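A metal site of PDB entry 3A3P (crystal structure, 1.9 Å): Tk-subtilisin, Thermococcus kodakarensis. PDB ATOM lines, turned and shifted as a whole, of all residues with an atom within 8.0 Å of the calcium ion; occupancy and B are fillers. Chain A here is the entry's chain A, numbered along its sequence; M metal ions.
Six residues have an atom within 4 Å of the calcium ion: Gln 15, Asp 55, Leu 95, Asn 97, Ile 99 and Val 101.
The nearest printed residue that does not touch the calcium ion is Gly 100 (4.3 Å).
The backbone carbonyl oxygen (O) of Val 101 binds the calcium ion (2.3 Å).
The calcium ion is bound by O of Leu 95 (2.3 Å).
OD1 of Asn 97 binds the calcium ion.
O of Ile 99 is bound to the calcium ion, at 2.4 Å.
The calcium ion is bound by OD1 of Asp 55, at 2.4 Å.
The calcium ion is bound by the side-chain amide oxygen (OE1) of Gln 15, at 2.5 Å.
OD2 of Asp 55 is bound to the calcium ion, at 2.6 Å.
The calcium ion has seven donor atoms within binding distance.
The side-chain amide nitrogen (NE2) of Gln 15 is in hydrogen-bond range of the side-chain amide oxygen (OD1) of Asn 96.
N of Gln 15 lies within hydrogen-bond range of O of Asp 98, 3.1 Å away.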
ATOM      1  N   GLN A  12      12.823 -28.016 -12.057  1.00  0.00           N
ATOM      2  CA  GLN A  12      12.762 -26.570 -11.590  1.00  0.00           C
ATOM      3  C   GLN A  12      13.608 -26.300 -10.348  1.00  0.00           C
ATOM      4  O   GLN A  12      13.544 -27.061  -9.391  1.00  0.00           O
ATOM      5  CB  GLN A  12      11.312 -26.143 -11.322  1.00  0.00           C
ATOM      6  CG  GLN A  12      10.446 -26.075 -12.569  1.00  0.00           C
ATOM      7  CD  GLN A  12      10.801 -24.880 -13.430  1.00  0.00           C
ATOM      8  OE1 GLN A  12      10.970 -23.757 -12.929  1.00  0.00           O
ATOM      9  NE2 GLN A  12      10.910 -25.111 -14.724  1.00  0.00           N
ATOM     10  N   PRO A  13      14.386 -25.200 -10.367  1.00  0.00           N
ATOM     11  CA  PRO A  13      15.206 -24.818  -9.203  1.00  0.00           C
ATOM     12  C   PRO A  13      14.338 -24.271  -8.057  1.00  0.00           C
ATOM     13  O   PRO A  13      13.283 -23.697  -8.323  1.00  0.00           O
ATOM     14  CB  PRO A  13      16.128 -23.717  -9.755  1.00  0.00           C
ATOM     15  CG  PRO A  13      15.342 -23.115 -10.873  1.00  0.00           C
ATOM     16  CD  PRO A  13      14.555 -24.263 -11.490  1.00  0.00           C
ATOM     17  N   ALA A  14      14.767 -24.451  -6.799  1.00  0.00           N
ATOM     18  CA  ALA A  14      14.126 -23.814  -5.654  1.00  0.00           C
ATOM     19  C   ALA A  14      14.063 -22.283  -5.829  1.00  0.00           C
ATOM     20  O   ALA A  14      14.935 -21.711  -6.451  1.00  0.00           O
ATOM     21  CB  ALA A  14      14.909 -24.149  -4.368  1.00  0.00           C
ATOM     22  N   GLN A  15      13.053 -21.647  -5.255  1.00  0.00           N
ATOM     23  CA  GLN A  15      12.824 -20.222  -5.489  1.00  0.00           C
ATOM     24  C   GLN A  15      13.866 -19.342  -4.827  1.00  0.00           C
ATOM     25  O   GLN A  15      14.221 -19.602  -3.675  1.00  0.00           O
ATOM     26  CB  GLN A  15      11.425 -19.814  -5.036  1.00  0.00           C
ATOM     27  CG  GLN A  15      11.157 -18.301  -5.168  1.00  0.00           C
ATOM     28  CD  GLN A  15       9.728 -17.943  -4.891  1.00  0.00           C
ATOM     29  OE1 GLN A  15       8.860 -18.120  -5.748  1.00  0.00           O
ATOM     30  NE2 GLN A  15       9.466 -17.429  -3.700  1.00  0.00           N
ATOM     31  N   THR A  16      14.352 -18.335  -5.550  1.00  0.00           N
ATOM     32  CA  THR A  16      15.066 -17.197  -4.951  1.00  0.00           C
ATOM     33  C   THR A  16      14.384 -15.886  -5.198  1.00  0.00           C
ATOM     34  O   THR A  16      13.639 -15.752  -6.174  1.00  0.00           O
ATOM     35  CB  THR A  16      16.458 -16.857  -5.586  1.00  0.00           C
ATOM     36  OG1 THR A  16      16.617 -17.419  -6.909  1.00  0.00           O
ATOM     37  CG2 THR A  16      17.553 -17.160  -4.688  1.00  0.00           C
ATOM     38  N   HIS A  53       5.204 -21.311 -18.988  1.00  0.00           N
ATOM     39  CA  HIS A  53       6.247 -21.305 -17.982  1.00  0.00           C
ATOM     40  C   HIS A  53       5.649 -21.588 -16.611  1.00  0.00           C
ATOM     41  O   HIS A  53       4.763 -20.870 -16.165  1.00  0.00           O
ATOM     42  CB  HIS A  53       7.029 -19.964 -17.947  1.00  0.00           C
ATOM     43  CG  HIS A  53       8.275 -20.045 -17.118  1.00  0.00           C
ATOM     44  ND1 HIS A  53       9.543 -19.869 -17.631  1.00  0.00           N
ATOM     45  CD2 HIS A  53       8.453 -20.326 -15.803  1.00  0.00           C
ATOM     46  CE1 HIS A  53      10.441 -19.997 -16.671  1.00  0.00           C
ATOM     47  NE2 HIS A  53       9.811 -20.286 -15.555  1.00  0.00           N
ATOM     48  N   PRO A  54       6.167 -22.614 -15.902  1.00  0.00           N
ATOM     49  CA  PRO A  54       5.638 -22.967 -14.594  1.00  0.00           C
ATOM     50  C   PRO A  54       5.623 -21.790 -13.594  1.00  0.00           C
ATOM     51  O   PRO A  54       4.777 -21.755 -12.686  1.00  0.00           O
ATOM     52  CB  PRO A  54       6.582 -24.077 -14.113  1.00  0.00           C
ATOM     53  CG  PRO A  54       7.152 -24.702 -15.356  1.00  0.00           C
ATOM     54  CD  PRO A  54       7.275 -23.506 -16.323  1.00  0.00           C
ATOM     55  N   ASP A  55       6.511 -20.822 -13.754  1.00  0.00           N
ATOM     56  CA  ASP A  55       6.576 -19.722 -12.784  1.00  0.00           C
ATOM     57  C   ASP A  55       5.835 -18.470 -13.235  1.00  0.00           C
ATOM     58  O   ASP A  55       5.914 -17.409 -12.585  1.00  0.00           O
ATOM     59  CB  ASP A  55       8.045 -19.402 -12.434  1.00  0.00           C
ATOM     60  CG  ASP A  55       8.226 -19.038 -10.978  1.00  0.00           C
ATOM     61  OD1 ASP A  55       7.418 -19.482 -10.134  1.00  0.00           O
ATOM     62  OD2 ASP A  55       9.177 -18.315 -10.650  1.00  0.00           O
ATOM     63  N   LEU A  56       5.119 -18.604 -14.352  1.00  0.00           N
ATOM     64  CA  LEU A  56       4.366 -17.503 -14.954  1.00  0.00           C
ATOM     65  C   LEU A  56       2.912 -17.822 -15.270  1.00  0.00           C
ATOM     66  O   LEU A  56       2.051 -16.927 -15.215  1.00  0.00           O
ATOM     67  CB  LEU A  56       5.026 -17.067 -16.266  1.00  0.00           C
ATOM     68  CG  LEU A  56       6.456 -16.516 -16.285  1.00  0.00           C
ATOM     69  CD1 LEU A  56       6.688 -16.029 -17.713  1.00  0.00           C
ATOM     70  CD2 LEU A  56       6.640 -15.356 -15.293  1.00  0.00           C
ATOM     71  N   ALA A  93       5.862 -10.325 -12.443  1.00  0.00           N
ATOM     72  CA  ALA A  93       4.777 -11.214 -11.993  1.00  0.00           C
ATOM     73  C   ALA A  93       5.128 -12.687 -11.848  1.00  0.00           C
ATOM     74  O   ALA A  93       4.209 -13.515 -11.807  1.00  0.00           O
ATOM     75  CB  ALA A  93       3.536 -11.061 -12.897  1.00  0.00           C
ATOM     76  N   ALA A  94       6.417 -13.036 -11.744  1.00  0.00           N
ATOM     77  CA  ALA A  94       6.748 -14.456 -11.434  1.00  0.00           C
ATOM     78  C   ALA A  94       6.113 -14.828 -10.101  1.00  0.00           C
ATOM     79  O   ALA A  94       6.103 -14.035  -9.186  1.00  0.00           O
ATOM     80  CB  ALA A  94       8.278 -14.710 -11.390  1.00  0.00           C
ATOM     81  N   LEU A  95       5.549 -16.022 -10.020  1.00  0.00           N
ATOM     82  CA  LEU A  95       4.708 -16.415  -8.901  1.00  0.00           C
ATOM     83  C   LEU A  95       5.553 -16.626  -7.641  1.00  0.00           C
ATOM     84  O   LEU A  95       6.722 -17.019  -7.734  1.00  0.00           O
ATOM     85  CB  LEU A  95       3.990 -17.718  -9.299  1.00  0.00           C
ATOM     86  CG  LEU A  95       2.936 -17.522 -10.383  1.00  0.00           C
ATOM     87  CD1 LEU A  95       2.750 -18.793 -11.262  1.00  0.00           C
ATOM     88  CD2 LEU A  95       1.642 -17.095  -9.749  1.00  0.00           C
ATOM     89  N   ASN A  96       4.962 -16.368  -6.488  1.00  0.00           N
ATOM     90  CA  ASN A  96       5.604 -16.604  -5.205  1.00  0.00           C
ATOM     91  C   ASN A  96       5.205 -18.015  -4.786  1.00  0.00           C
ATOM     92  O   ASN A  96       4.095 -18.232  -4.322  1.00  0.00           O
ATOM     93  CB  ASN A  96       5.104 -15.599  -4.190  1.00  0.00           C
ATOM     94  CG  ASN A  96       5.869 -15.623  -2.860  1.00  0.00           C
ATOM     95  OD1 ASN A  96       6.802 -16.394  -2.681  1.00  0.00           O
ATOM     96  ND2 ASN A  96       5.476 -14.774  -1.957  1.00  0.00           N
ATOM     97  N   ASN A  97       6.115 -18.953  -4.978  1.00  0.00           N
ATOM     98  CA  ASN A  97       5.825 -20.394  -4.815  1.00  0.00           C
ATOM     99  C   ASN A  97       7.123 -21.082  -4.400  1.00  0.00           C
ATOM    100  O   ASN A  97       7.975 -20.451  -3.773  1.00  0.00           O
ATOM    101  CB  ASN A  97       5.246 -21.003  -6.118  1.00  0.00           C
ATOM    102  CG  ASN A  97       6.106 -20.711  -7.365  1.00  0.00           C
ATOM    103  OD1 ASN A  97       7.280 -20.383  -7.269  1.00  0.00           O
ATOM    104  ND2 ASN A  97       5.513 -20.866  -8.548  1.00  0.00           N
ATOM    105  N   ASP A  98       7.318 -22.334  -4.787  1.00  0.00           N
ATOM    106  CA  ASP A  98       8.557 -23.001  -4.414  1.00  0.00           C
ATOM    107  C   ASP A  98       9.661 -23.081  -5.453  1.00  0.00           C
ATOM    108  O   ASP A  98      10.697 -23.700  -5.205  1.00  0.00           O
ATOM    109  CB  ASP A  98       8.253 -24.346  -3.751  1.00  0.00           C
ATOM    110  CG  ASP A  98       7.492 -24.163  -2.437  1.00  0.00           C
ATOM    111  OD1 ASP A  98       8.110 -23.731  -1.409  1.00  0.00           O
ATOM    112  OD2 ASP A  98       6.249 -24.395  -2.428  1.00  0.00           O
ATOM    113  N   ILE A  99       9.470 -22.434  -6.614  1.00  0.00           N
ATOM    114  CA  ILE A  99      10.420 -22.540  -7.711  1.00  0.00           C
ATOM    115  C   ILE A  99      10.859 -21.179  -8.290  1.00  0.00           C
ATOM    116  O   ILE A  99      10.190 -20.161  -8.127  1.00  0.00           O
ATOM    117  CB  ILE A  99       9.804 -23.378  -8.889  1.00  0.00           C
ATOM    118  CG1 ILE A  99       8.469 -22.760  -9.329  1.00  0.00           C
ATOM    119  CG2 ILE A  99       9.528 -24.855  -8.437  1.00  0.00           C
ATOM    120  CD1 ILE A  99       8.041 -23.123 -10.719  1.00  0.00           C
ATOM    121  N   GLY A 100      11.966 -21.194  -9.002  1.00  0.00           N
ATOM    122  CA  GLY A 100      12.331 -20.101  -9.891  1.00  0.00           C
ATOM    123  C   GLY A 100      12.594 -18.793  -9.186  1.00  0.00           C
ATOM    124  O   GLY A 100      13.473 -18.683  -8.322  1.00  0.00           O
ATOM    125  N   VAL A 101      11.881 -17.760  -9.609  1.00  0.00           N
ATOM    126  CA  VAL A 101      12.078 -16.439  -9.022  1.00  0.00           C
ATOM    127  C   VAL A 101      10.768 -15.917  -8.434  1.00  0.00           C
ATOM    128  O   VAL A 101       9.858 -16.712  -8.141  1.00  0.00           O
ATOM    129  CB  VAL A 101      12.683 -15.467 -10.061  1.00  0.00           C
ATOM    130  CG1 VAL A 101      14.118 -15.908 -10.426  1.00  0.00           C
ATOM    131  CG2 VAL A 101      11.791 -15.381 -11.312  1.00  0.00           C
ATOM    132  N   VAL A 102      10.630 -14.600  -8.234  1.00  0.00           N
ATOM    133  CA  VAL A 102       9.357 -14.030  -7.758  1.00  0.00           C
ATOM    134  C   VAL A 102       9.318 -12.598  -8.287  1.00  0.00           C
ATOM    135  O   VAL A 102      10.350 -11.925  -8.316  1.00  0.00           O
ATOM    136  CB  VAL A 102       9.154 -14.127  -6.196  1.00  0.00           C
ATOM    137  CG1 VAL A 102      10.310 -13.485  -5.384  1.00  0.00           C
ATOM    138  CG2 VAL A 102       7.803 -13.536  -5.725  1.00  0.00           C
ATOM    139  N   GLY A 103       8.145 -12.159  -8.778  1.00  0.00           N
ATOM    140  CA  GLY A 103       8.099 -10.814  -9.338  1.00  0.00           C
ATOM    141  C   GLY A 103       7.838  -9.783  -8.265  1.00  0.00           C
ATOM    142  O   GLY A 103       7.563 -10.144  -7.125  1.00  0.00           O
ATOM    143  N   PRO A 106       3.785 -10.514  -7.388  1.00  0.00           N
ATOM    144  CA  PRO A 106       3.711 -11.913  -7.800  1.00  0.00           C
ATOM    145  C   PRO A 106       2.283 -12.496  -7.989  1.00  0.00           C
ATOM    146  O   PRO A 106       2.155 -13.659  -8.433  1.00  0.00           O
ATOM    147  CB  PRO A 106       4.477 -12.648  -6.667  1.00  0.00           C
ATOM    148  CG  PRO A 106       4.439 -11.778  -5.515  1.00  0.00           C
ATOM    149  CD  PRO A 106       4.288 -10.345  -6.009  1.00  0.00           C
ATOM    150  N   THR A 242      12.643 -15.135 -15.390  1.00  0.00           N
ATOM    151  CA  THR A 242      12.213 -16.235 -16.238  1.00  0.00           C
ATOM    152  C   THR A 242      12.689 -16.057 -17.678  1.00  0.00           C
ATOM    153  O   THR A 242      12.886 -14.938 -18.181  1.00  0.00           O
ATOM    154  CB  THR A 242      10.674 -16.343 -16.215  1.00  0.00           C
ATOM    155  OG1 THR A 242      10.109 -15.016 -16.340  1.00  0.00           O
ATOM    156  CG2 THR A 242      10.193 -16.952 -14.877  1.00  0.00           C
ATOM    157  N   TYR A 248      15.435 -19.867 -16.774  1.00  0.00           N
ATOM    158  CA  TYR A 248      15.793 -18.573 -16.131  1.00  0.00           C
ATOM    159  C   TYR A 248      17.091 -18.066 -16.752  1.00  0.00           C
ATOM    160  O   TYR A 248      17.904 -18.859 -17.201  1.00  0.00           O
ATOM    161  CB  TYR A 248      15.935 -18.751 -14.609  1.00  0.00           C
ATOM    162  CG  TYR A 248      14.727 -19.428 -14.044  1.00  0.00           C
ATOM    163  CD1 TYR A 248      14.626 -20.832 -14.029  1.00  0.00           C
ATOM    164  CD2 TYR A 248      13.650 -18.682 -13.609  1.00  0.00           C
ATOM    165  CE1 TYR A 248      13.476 -21.456 -13.570  1.00  0.00           C
ATOM    166  CE2 TYR A 248      12.505 -19.287 -13.147  1.00  0.00           C
ATOM    167  CZ  TYR A 248      12.418 -20.683 -13.139  1.00  0.00           C
ATOM    168  OH  TYR A 248      11.247 -21.261 -12.670  1.00  0.00           O
HETATM  169 CA    CA M   1       8.464 -18.541  -8.136  1.00  0.00          CA
